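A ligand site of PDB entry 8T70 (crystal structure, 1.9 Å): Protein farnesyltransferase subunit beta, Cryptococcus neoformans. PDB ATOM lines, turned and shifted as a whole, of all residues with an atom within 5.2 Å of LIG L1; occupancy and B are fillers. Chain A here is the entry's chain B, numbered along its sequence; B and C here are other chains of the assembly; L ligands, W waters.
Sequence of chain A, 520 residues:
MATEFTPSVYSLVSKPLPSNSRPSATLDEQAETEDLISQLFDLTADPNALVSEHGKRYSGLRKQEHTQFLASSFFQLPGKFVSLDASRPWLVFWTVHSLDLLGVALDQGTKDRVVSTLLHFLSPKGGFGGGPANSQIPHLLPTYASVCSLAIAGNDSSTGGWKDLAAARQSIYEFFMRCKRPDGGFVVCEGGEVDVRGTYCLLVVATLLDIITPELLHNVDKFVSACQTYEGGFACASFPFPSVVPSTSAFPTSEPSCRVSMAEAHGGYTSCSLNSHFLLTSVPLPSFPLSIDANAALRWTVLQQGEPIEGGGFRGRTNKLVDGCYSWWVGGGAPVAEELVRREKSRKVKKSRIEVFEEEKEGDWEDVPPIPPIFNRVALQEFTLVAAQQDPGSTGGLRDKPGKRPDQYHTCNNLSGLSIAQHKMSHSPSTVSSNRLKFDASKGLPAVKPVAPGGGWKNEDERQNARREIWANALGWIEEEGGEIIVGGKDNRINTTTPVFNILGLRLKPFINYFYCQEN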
ATOM      1  N   TRP A  90      24.287  19.238 -14.102  1.00  0.00           N
ATOM      2  CA  TRP A  90      24.073  20.404 -14.956  1.00  0.00           C
ATOM      3  C   TRP A  90      25.387  21.111 -15.250  1.00  0.00           C
ATOM      4  O   TRP A  90      25.608  21.570 -16.378  1.00  0.00           O
ATOM      5  CB  TRP A  90      23.084  21.369 -14.304  1.00  0.00           C
ATOM      6  CG  TRP A  90      21.692  20.845 -14.354  1.00  0.00           C
ATOM      7  CD1 TRP A  90      20.957  20.320 -13.318  1.00  0.00           C
ATOM      8  CD2 TRP A  90      20.860  20.770 -15.505  1.00  0.00           C
ATOM      9  NE1 TRP A  90      19.720  19.929 -13.778  1.00  0.00           N
ATOM     10  CE2 TRP A  90      19.637  20.196 -15.111  1.00  0.00           C
ATOM     11  CE3 TRP A  90      21.035  21.156 -16.847  1.00  0.00           C
ATOM     12  CZ2 TRP A  90      18.590  19.999 -16.004  1.00  0.00           C
ATOM     13  CZ3 TRP A  90      19.997  20.947 -17.727  1.00  0.00           C
ATOM     14  CH2 TRP A  90      18.795  20.367 -17.320  1.00  0.00           C
ATOM     15  N   LEU A 141      15.720  16.015 -13.011  1.00  0.00           N
ATOM     16  CA  LEU A 141      16.475  17.016 -13.776  1.00  0.00           C
ATOM     17  C   LEU A 141      17.938  16.583 -13.924  1.00  0.00           C
ATOM     18  O   LEU A 141      18.440  16.565 -15.059  1.00  0.00           O
ATOM     19  CB  LEU A 141      16.326  18.386 -13.131  1.00  0.00           C
ATOM     20  CG  LEU A 141      15.124  19.181 -13.672  1.00  0.00           C
ATOM     21  CD1 LEU A 141      13.789  18.421 -13.542  1.00  0.00           C
ATOM     22  CD2 LEU A 141      15.026  20.504 -12.954  1.00  0.00           C
ATOM     23  N   ARG A 197       9.123  21.043 -15.934  1.00  0.00           N
ATOM     24  CA  ARG A 197      10.551  20.700 -16.034  1.00  0.00           C
ATOM     25  C   ARG A 197      10.737  19.198 -15.881  1.00  0.00           C
ATOM     26  O   ARG A 197      11.483  18.564 -16.636  1.00  0.00           O
ATOM     27  CB  ARG A 197      11.384  21.409 -14.941  1.00  0.00           C
ATOM     28  CG  ARG A 197      11.570  22.916 -15.057  1.00  0.00           C
ATOM     29  CD  ARG A 197      12.172  23.469 -13.761  1.00  0.00           C
ATOM     30  NE  ARG A 197      11.433  22.965 -12.594  1.00  0.00           N
ATOM     31  CZ  ARG A 197      11.991  22.562 -11.466  1.00  0.00           C
ATOM     32  NH1 ARG A 197      13.301  22.696 -11.248  1.00  0.00           N
ATOM     33  NH2 ARG A 197      11.240  21.983 -10.536  1.00  0.00           N
ATOM     34  N   TYR A 200       9.370  17.375 -18.979  1.00  0.00           N
ATOM     35  CA  TYR A 200      10.319  17.483 -20.101  1.00  0.00           C
ATOM     36  C   TYR A 200      11.508  16.547 -19.894  1.00  0.00           C
ATOM     37  O   TYR A 200      11.844  15.754 -20.779  1.00  0.00           O
ATOM     38  CB  TYR A 200      10.792  18.925 -20.242  1.00  0.00           C
ATOM     39  CG  TYR A 200      12.017  19.027 -21.151  1.00  0.00           C
ATOM     40  CD1 TYR A 200      11.902  18.919 -22.520  1.00  0.00           C
ATOM     41  CD2 TYR A 200      13.305  19.194 -20.605  1.00  0.00           C
ATOM     42  CE1 TYR A 200      13.038  18.998 -23.363  1.00  0.00           C
ATOM     43  CE2 TYR A 200      14.438  19.266 -21.435  1.00  0.00           C
ATOM     44  CZ  TYR A 200      14.285  19.179 -22.806  1.00  0.00           C
ATOM     45  OH  TYR A 200      15.413  19.259 -23.625  1.00  0.00           O
ATOM     46  N   CYS A 201      12.152  16.647 -18.732  1.00  0.00           N
ATOM     47  CA  CYS A 201      13.350  15.848 -18.504  1.00  0.00           C
ATOM     48  C   CYS A 201      13.055  14.359 -18.593  1.00  0.00           C
ATOM     49  O   CYS A 201      13.843  13.598 -19.143  1.00  0.00           O
ATOM     50  CB  CYS A 201      13.953  16.201 -17.141  1.00  0.00           C
ATOM     51  SG  CYS A 201      14.734  17.823 -17.122  1.00  0.00           S
ATOM     52  N   HIS A 266       5.984  31.463 -19.139  1.00  0.00           N
ATOM     53  CA  HIS A 266       7.398  31.731 -18.889  1.00  0.00           C
ATOM     54  C   HIS A 266       8.230  30.966 -19.909  1.00  0.00           C
ATOM     55  O   HIS A 266       7.915  29.821 -20.253  1.00  0.00           O
ATOM     56  CB  HIS A 266       7.795  31.325 -17.469  1.00  0.00           C
ATOM     57  CG  HIS A 266       9.195  31.711 -17.109  1.00  0.00           C
ATOM     58  ND1 HIS A 266       9.501  32.856 -16.416  1.00  0.00           N
ATOM     59  CD2 HIS A 266      10.383  31.115 -17.389  1.00  0.00           C
ATOM     60  CE1 HIS A 266      10.812  32.941 -16.263  1.00  0.00           C
ATOM     61  NE2 HIS A 266      11.374  31.893 -16.851  1.00  0.00           N
ATOM     62  N   GLY A 268      11.110  29.476 -19.764  1.00  0.00           N
ATOM     63  CA  GLY A 268      11.601  28.178 -19.305  1.00  0.00           C
ATOM     64  C   GLY A 268      10.541  27.093 -19.353  1.00  0.00           C
ATOM     65  O   GLY A 268      10.770  26.001 -19.869  1.00  0.00           O
ATOM     66  N   TYR A 269       9.355  27.389 -18.809  1.00  0.00           N
ATOM     67  CA  TYR A 269       8.302  26.379 -18.818  1.00  0.00           C
ATOM     68  C   TYR A 269       7.648  26.259 -20.182  1.00  0.00           C
ATOM     69  O   TYR A 269       7.119  25.182 -20.502  1.00  0.00           O
ATOM     70  CB  TYR A 269       7.277  26.706 -17.728  1.00  0.00           C
ATOM     71  CG  TYR A 269       7.900  26.756 -16.352  1.00  0.00           C
ATOM     72  CD1 TYR A 269       8.485  25.626 -15.806  1.00  0.00           C
ATOM     73  CD2 TYR A 269       7.912  27.928 -15.607  1.00  0.00           C
ATOM     74  CE1 TYR A 269       9.066  25.662 -14.555  1.00  0.00           C
ATOM     75  CE2 TYR A 269       8.489  27.970 -14.363  1.00  0.00           C
ATOM     76  CZ  TYR A 269       9.058  26.837 -13.840  1.00  0.00           C
ATOM     77  OH  TYR A 269       9.618  26.880 -12.584  1.00  0.00           O
ATOM     78  N   CYS A 272       9.885  23.784 -21.997  1.00  0.00           N
ATOM     79  CA  CYS A 272       9.630  22.434 -21.508  1.00  0.00           C
ATOM     80  C   CYS A 272       8.277  21.917 -21.983  1.00  0.00           C
ATOM     81  O   CYS A 272       8.143  20.735 -22.313  1.00  0.00           O
ATOM     82  CB  CYS A 272       9.705  22.408 -19.979  1.00  0.00           C
ATOM     83  SG  CYS A 272      11.380  22.656 -19.364  1.00  0.00           S
ATOM     84  N   GLY A 316      11.871  36.435 -20.815  1.00  0.00           N
ATOM     85  CA  GLY A 316      11.261  35.180 -20.414  1.00  0.00           C
ATOM     86  C   GLY A 316       9.788  35.312 -20.072  1.00  0.00           C
ATOM     87  O   GLY A 316       9.082  34.300 -19.991  1.00  0.00           O
ATOM     88  N   ARG A 317       9.323  36.538 -19.857  1.00  0.00           N
ATOM     89  CA  ARG A 317       7.894  36.756 -19.663  1.00  0.00           C
ATOM     90  C   ARG A 317       7.590  38.225 -19.892  1.00  0.00           C
ATOM     91  O   ARG A 317       8.473  39.089 -19.803  1.00  0.00           O
ATOM     92  CB  ARG A 317       7.419  36.280 -18.287  1.00  0.00           C
ATOM     93  CG  ARG A 317       8.366  36.535 -17.143  1.00  0.00           C
ATOM     94  CD  ARG A 317       7.793  36.011 -15.796  1.00  0.00           C
ATOM     95  NE  ARG A 317       8.876  35.954 -14.819  1.00  0.00           N
ATOM     96  CZ  ARG A 317       8.719  36.120 -13.505  1.00  0.00           C
ATOM     97  NH1 ARG A 317       7.520  36.300 -12.973  1.00  0.00           N
ATOM     98  NH2 ARG A 317       9.794  36.120 -12.731  1.00  0.00           N
ATOM     99  N   LYS A 320       9.129  41.792 -18.350  1.00  0.00           N
ATOM    100  CA  LYS A 320      10.392  41.568 -17.659  1.00  0.00           C
ATOM    101  C   LYS A 320      11.539  41.832 -18.637  1.00  0.00           C
ATOM    102  O   LYS A 320      11.315  42.259 -19.764  1.00  0.00           O
ATOM    103  CB  LYS A 320      10.425  40.164 -17.075  1.00  0.00           C
ATOM    104  CG  LYS A 320       9.299  39.939 -16.072  1.00  0.00           C
ATOM    105  CD  LYS A 320       9.812  40.289 -14.731  1.00  0.00           C
ATOM    106  CE  LYS A 320      10.355  39.091 -14.068  1.00  0.00           C
ATOM    107  NZ  LYS A 320      11.480  39.448 -13.145  1.00  0.00           N
ATOM    108  N   LEU A 321      12.759  41.552 -18.207  1.00  0.00           N
ATOM    109  CA  LEU A 321      13.953  41.984 -18.941  1.00  0.00           C
ATOM    110  C   LEU A 321      14.472  40.885 -19.877  1.00  0.00           C
ATOM    111  O   LEU A 321      14.337  39.693 -19.609  1.00  0.00           O
ATOM    112  CB  LEU A 321      15.049  42.397 -17.960  1.00  0.00           C
ATOM    113  CG  LEU A 321      14.677  43.422 -16.883  1.00  0.00           C
ATOM    114  CD1 LEU A 321      15.839  43.601 -15.913  1.00  0.00           C
ATOM    115  CD2 LEU A 321      14.322  44.761 -17.534  1.00  0.00           C
ATOM    116  N   ASP A 323      17.248  38.498 -21.532  1.00  0.00           N
ATOM    117  CA  ASP A 323      18.248  37.684 -20.842  1.00  0.00           C
ATOM    118  C   ASP A 323      18.748  36.636 -21.825  1.00  0.00           C
ATOM    119  O   ASP A 323      17.934  35.914 -22.428  1.00  0.00           O
ATOM    120  CB  ASP A 323      17.637  37.051 -19.577  1.00  0.00           C
ATOM    121  CG  ASP A 323      18.567  36.066 -18.869  1.00  0.00           C
ATOM    122  OD1 ASP A 323      19.624  35.666 -19.429  1.00  0.00           O
ATOM    123  OD2 ASP A 323      18.243  35.685 -17.718  1.00  0.00           O
ATOM    124  N   TYR A 326      17.381  32.990 -22.438  1.00  0.00           N
ATOM    125  CA  TYR A 326      16.153  32.768 -23.187  1.00  0.00           C
ATOM    126  C   TYR A 326      16.375  32.678 -24.689  1.00  0.00           C
ATOM    127  O   TYR A 326      15.426  32.379 -25.422  1.00  0.00           O
ATOM    128  CB  TYR A 326      15.125  33.867 -22.890  1.00  0.00           C
ATOM    129  CG  TYR A 326      14.740  33.892 -21.439  1.00  0.00           C
ATOM    130  CD1 TYR A 326      14.211  32.760 -20.830  1.00  0.00           C
ATOM    131  CD2 TYR A 326      14.934  35.029 -20.663  1.00  0.00           C
ATOM    132  CE1 TYR A 326      13.871  32.768 -19.487  1.00  0.00           C
ATOM    133  CE2 TYR A 326      14.597  35.044 -19.315  1.00  0.00           C
ATOM    134  CZ  TYR A 326      14.060  33.909 -18.735  1.00  0.00           C
ATOM    135  OH  TYR A 326      13.707  33.922 -17.410  1.00  0.00           O
ATOM    136  N   TRP A 329      15.746  29.024 -24.309  1.00  0.00           N
ATOM    137  CA  TRP A 329      14.413  28.642 -23.823  1.00  0.00           C
ATOM    138  C   TRP A 329      13.316  29.136 -24.763  1.00  0.00           C
ATOM    139  O   TRP A 329      12.379  28.390 -25.073  1.00  0.00           O
ATOM    140  CB  TRP A 329      14.175  29.171 -22.407  1.00  0.00           C
ATOM    141  CG  TRP A 329      15.164  28.629 -21.425  1.00  0.00           C
ATOM    142  CD1 TRP A 329      16.025  29.336 -20.635  1.00  0.00           C
ATOM    143  CD2 TRP A 329      15.429  27.240 -21.169  1.00  0.00           C
ATOM    144  NE1 TRP A 329      16.810  28.472 -19.898  1.00  0.00           N
ATOM    145  CE2 TRP A 329      16.459  27.188 -20.198  1.00  0.00           C
ATOM    146  CE3 TRP A 329      14.894  26.047 -21.646  1.00  0.00           C
ATOM    147  CZ2 TRP A 329      16.951  25.985 -19.708  1.00  0.00           C
ATOM    148  CZ3 TRP A 329      15.386  24.844 -21.156  1.00  0.00           C
ATOM    149  CH2 TRP A 329      16.415  24.818 -20.205  1.00  0.00           C
ATOM    150  N   TYR A 409      25.797  28.061 -16.992  1.00  0.00           N
ATOM    151  CA  TYR A 409      24.418  27.984 -17.466  1.00  0.00           C
ATOM    152  C   TYR A 409      24.160  28.970 -18.609  1.00  0.00           C
ATOM    153  O   TYR A 409      23.594  28.594 -19.645  1.00  0.00           O
ATOM    154  CB  TYR A 409      23.489  28.258 -16.290  1.00  0.00           C
ATOM    155  CG  TYR A 409      22.071  28.609 -16.673  1.00  0.00           C
ATOM    156  CD1 TYR A 409      21.188  27.626 -17.099  1.00  0.00           C
ATOM    157  CD2 TYR A 409      21.611  29.923 -16.577  1.00  0.00           C
ATOM    158  CE1 TYR A 409      19.865  27.949 -17.433  1.00  0.00           C
ATOM    159  CE2 TYR A 409      20.297  30.245 -16.918  1.00  0.00           C
ATOM    160  CZ  TYR A 409      19.434  29.255 -17.349  1.00  0.00           C
ATOM    161  OH  TYR A 409      18.132  29.569 -17.706  1.00  0.00           O
ATOM    162  N   TYR B 123      13.647  26.429  -5.139  1.00  0.00           N
ATOM    163  CA  TYR B 123      12.509  25.549  -5.462  1.00  0.00           C
ATOM    164  C   TYR B 123      12.234  24.687  -4.228  1.00  0.00           C
ATOM    165  O   TYR B 123      11.081  24.347  -3.992  1.00  0.00           O
ATOM    166  CB  TYR B 123      12.875  24.583  -6.585  1.00  0.00           C
ATOM    167  CG  TYR B 123      12.647  25.066  -7.997  1.00  0.00           C
ATOM    168  CD1 TYR B 123      11.410  24.959  -8.596  1.00  0.00           C
ATOM    169  CD2 TYR B 123      13.692  25.579  -8.738  1.00  0.00           C
ATOM    170  CE1 TYR B 123      11.196  25.389  -9.897  1.00  0.00           C
ATOM    171  CE2 TYR B 123      13.507  26.018 -10.035  1.00  0.00           C
ATOM    172  CZ  TYR B 123      12.257  25.919 -10.617  1.00  0.00           C
ATOM    173  OH  TYR B 123      12.057  26.344 -11.901  1.00  0.00           O
ATOM    174  N   TYR B 159       8.430  34.375  -9.284  1.00  0.00           N
ATOM    175  CA  TYR B 159       7.589  33.401  -9.978  1.00  0.00           C
ATOM    176  C   TYR B 159       7.128  32.291  -9.036  1.00  0.00           C
ATOM    177  O   TYR B 159       5.962  31.889  -9.054  1.00  0.00           O
ATOM    178  CB  TYR B 159       8.349  32.814 -11.178  1.00  0.00           C
ATOM    179  CG  TYR B 159       7.451  32.029 -12.100  1.00  0.00           C
ATOM    180  CD1 TYR B 159       7.078  30.726 -11.812  1.00  0.00           C
ATOM    181  CD2 TYR B 159       6.946  32.616 -13.253  1.00  0.00           C
ATOM    182  CE1 TYR B 159       6.229  30.007 -12.654  1.00  0.00           C
ATOM    183  CE2 TYR B 159       6.104  31.910 -14.101  1.00  0.00           C
ATOM    184  CZ  TYR B 159       5.747  30.610 -13.791  1.00  0.00           C
ATOM    185  OH  TYR B 159       4.905  29.919 -14.641  1.00  0.00           O
ATOM    186  N   HIS B 160       8.049  31.758  -8.218  1.00  0.00           N
ATOM    187  CA  HIS B 160       7.673  30.700  -7.282  1.00  0.00           C
ATOM    188  C   HIS B 160       6.599  31.175  -6.323  1.00  0.00           C
ATOM    189  O   HIS B 160       5.745  30.393  -5.899  1.00  0.00           O
ATOM    190  CB  HIS B 160       8.891  30.238  -6.468  1.00  0.00           C
ATOM    191  CG  HIS B 160      10.017  29.707  -7.282  1.00  0.00           C
ATOM    192  ND1 HIS B 160       9.848  28.815  -8.315  1.00  0.00           N
ATOM    193  CD2 HIS B 160      11.357  29.928  -7.201  1.00  0.00           C
ATOM    194  CE1 HIS B 160      11.021  28.514  -8.841  1.00  0.00           C
ATOM    195  NE2 HIS B 160      11.960  29.175  -8.179  1.00  0.00           N
ATOM    196  N   ILE C   5      19.975  28.906 -11.090  1.00  0.00           N
ATOM    197  CA  ILE C   5      18.977  28.155 -10.319  1.00  0.00           C
ATOM    198  C   ILE C   5      17.869  27.751 -11.284  1.00  0.00           C
ATOM    199  O   ILE C   5      16.886  28.459 -11.481  1.00  0.00           O
ATOM    200  CB  ILE C   5      18.440  28.960  -9.132  1.00  0.00           C
ATOM    201  CG1 ILE C   5      19.571  29.403  -8.206  1.00  0.00           C
ATOM    202  CG2 ILE C   5      17.403  28.138  -8.359  1.00  0.00           C
ATOM    203  CD1 ILE C   5      19.108  30.310  -7.076  1.00  0.00           C
ATOM    204  N   ILE C   6      18.023  26.558 -11.865  1.00  0.00           N
ATOM    205  CA  ILE C   6      16.959  25.938 -12.651  1.00  0.00           C
ATOM    206  C   ILE C   6      16.438  24.675 -12.007  1.00  0.00           C
ATOM    207  O   ILE C   6      15.549  24.025 -12.582  1.00  0.00           O
ATOM    208  CB  ILE C   6      17.402  25.680 -14.109  1.00  0.00           C
ATOM    209  CG1 ILE C   6      18.813  25.071 -14.163  1.00  0.00           C
ATOM    210  CG2 ILE C   6      17.361  26.977 -14.903  1.00  0.00           C
ATOM    211  CD1 ILE C   6      18.865  23.587 -13.873  1.00  0.00           C
HETATM  212  C1  LIG L   1      15.477  22.533 -15.957  1.00  0.00           C
HETATM  213  C2  LIG L   1      14.902  22.687 -17.367  1.00  0.00           C
HETATM  214  C3  LIG L   1      15.013  21.542 -18.371  1.00  0.00           C
HETATM  215  C4  LIG L   1      14.295  23.823 -17.722  1.00  0.00           C
HETATM  216  C5  LIG L   1      14.155  24.986 -16.743  1.00  0.00           C
HETATM  217  C6  LIG L   1      14.101  26.270 -17.588  1.00  0.00           C
HETATM  218  C7  LIG L   1      13.789  27.528 -16.820  1.00  0.00           C
HETATM  219  C8  LIG L   1      14.684  28.746 -17.028  1.00  0.00           C
HETATM  220  C9  LIG L   1      12.747  27.607 -15.995  1.00  0.00           C
HETATM  221  C10 LIG L   1      12.445  28.939 -15.269  1.00  0.00           C
HETATM  222  C11 LIG L   1      12.515  28.799 -13.741  1.00  0.00           C
HETATM  223  C12 LIG L   1      11.977  30.078 -13.049  1.00  0.00           C
HETATM  224  C13 LIG L   1      10.638  30.674 -13.493  1.00  0.00           C
HETATM  225  C14 LIG L   1      12.651  30.664 -12.082  1.00  0.00           C
HETATM  226  C15 LIG L   1      12.072  31.923 -11.445  1.00  0.00           C
HETATM  227  O1  LIG L   1      13.080  32.896 -11.223  1.00  0.00           O
HETATM  228  N1  LIG L   1      13.651  33.386 -12.416  1.00  0.00           N
HETATM  229  C16 LIG L   1      13.395  34.745 -12.895  1.00  0.00           C
HETATM  230  O2  LIG L   1      12.706  35.486 -12.292  1.00  0.00           O
HETATM  231  C17 LIG L   1      14.067  35.221 -14.186  1.00  0.00           C
HETATM  232  P1  LIG L   1      12.926  36.311 -15.193  1.00  0.00           P
HETATM  233  O3  LIG L   1      11.563  35.693 -15.402  1.00  0.00           O
HETATM  234  O4  LIG L   1      12.887  37.698 -14.621  1.00  0.00           O
HETATM  235  O5  LIG L   1      13.596  36.375 -16.546  1.00  0.00           O
HETATM  236  S1  LG2 L   2      18.747  33.406 -15.307  1.00  0.00           S
HETATM  237  C1  LG2 L   2      17.178  32.574 -14.981  1.00  0.00           C
HETATM  238  C2  LG2 L   2      16.158  32.587 -15.920  1.00  0.00           C
HETATM  239  C3  LG2 L   2      14.960  31.945 -15.640  1.00  0.00           C
HETATM  240  C4  LG2 L   2      14.818  31.312 -14.425  1.00  0.00           C
HETATM  241  C5  LG2 L   2      15.830  31.299 -13.481  1.00  0.00           C
HETATM  242  C6  LG2 L   2      17.024  31.934 -13.765  1.00  0.00           C
HETATM  243  O   HOH W   1      16.378  36.761 -16.320  1.00  0.00           O
HETATM  244  O   HOH W   2      10.930  32.633  -8.385  1.00  0.00           O
HETATM  245  O   HOH W   3      13.898  39.822 -15.944  1.00  0.00           O
HETATM  246  O   HOH W   4      12.413  37.828 -18.664  1.00  0.00           O
HETATM  247  O   HOH W   5      11.164  35.032 -10.223  1.00  0.00           O
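CD2 of Leu 141 touches C1 of LIG L1, 3.7 Å away.
Arg 197 touches LIG L1.
CD2 of Tyr 200 touches C3 of LIG L1, at 3.7 Å.
Cys 201 touches LIG L1 (SG to C3, 3.9 Å).
CE1 of His 266 touches O3 of LIG L1, at 3.0 Å.
Gly 268 touches LIG L1.
Tyr 269 touches LIG L1.
Cys 272 touches LIG L1 (SG to C4, 3.5 Å).
Trp 329 touches LIG L1.
Tyr 409 touches LIG L1 (OH to C8, 3.6 Å).
Tyr 123 of chain B touches LIG L1.
Tyr 159 of chain B touches LIG L1.
Ile 6 of chain C touches LIG L1 (O to C1, 3.7 Å).
Hydrophobic or aromatic side chains within 4 Å of LIG L1: Leu 141, Tyr 200, His 266, Tyr 269, Tyr 326, Trp 329, Tyr 159 of chain B and Ile 6 of chain C.
16 residues have an atom within 4 Å of LIG L1: Leu 141, Arg 197, Tyr 200, Cys 201, His 266, Gly 268, Tyr 269, Cys 272, Arg 317, Lys 320, Tyr 326, Trp 329, Tyr 409, Tyr 123 of chain B, Tyr 159 of chain B and Ile 6 of chain C.
The nearest printed residue that does not touch LIG L1 is Trp 90 (4.01 Å).
The indole nitrogen (NE1) of Trp 329 is in hydrogen-bond range of the side-chain hydroxyl (OH) of Tyr 409 (2.8 Å).
The side-chain hydroxyl of Tyr 123 of chain B is in hydrogen-bond range of the side-chain hydroxyl of Tyr 269, at 2.6 Å.
The backbone carbonyl oxygen of Gly 268 lies within hydrogen-bond range of the side-chain sulfur of Cys 272 (3.4 Å).
The side-chain hydroxyl (OH) of Tyr 326 is in hydrogen-bond range of a ring nitrogen (NE2) of His 266.
NH1 of Arg 197 is in hydrogen-bond range of O of Ile 6 of chain C (2.9 Å).
The backbone carbonyl oxygen (O) of Arg 197 lies within hydrogen-bond range of the side-chain sulfur (SG) of Cys 201, 3.4 Å away.
Water W5 lies within hydrogen-bond range of O2 of LIG L1 (2.6 Å), N of Tyr 159 of chain B (3.0 Å) and NH2 of Arg 317 (3.1 Å).
Water W3 lies within hydrogen-bond range of an oxygen (O4) of LIG L1 (2.7 Å) and the backbone NH of Leu 321 (3.1 Å).
Water W4 lies within hydrogen-bond range of the backbone NH (N) of Gly 316, an oxygen (O5) of LIG L1 and the backbone carbonyl oxygen (O) of Leu 321.
NZ of Lys 320 lies within salt-bridge range of O4 of LIG L1, 2.7 Å away.
An oxygen (O5) of LIG L1 lies within hydrogen-bond range of the side-chain hydroxyl (OH) of Tyr 326 (2.6 Å).
An oxygen (O3) of LIG L1 is in salt-bridge range of the guanidinium group (NE) of Arg 317 (2.8 Å).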
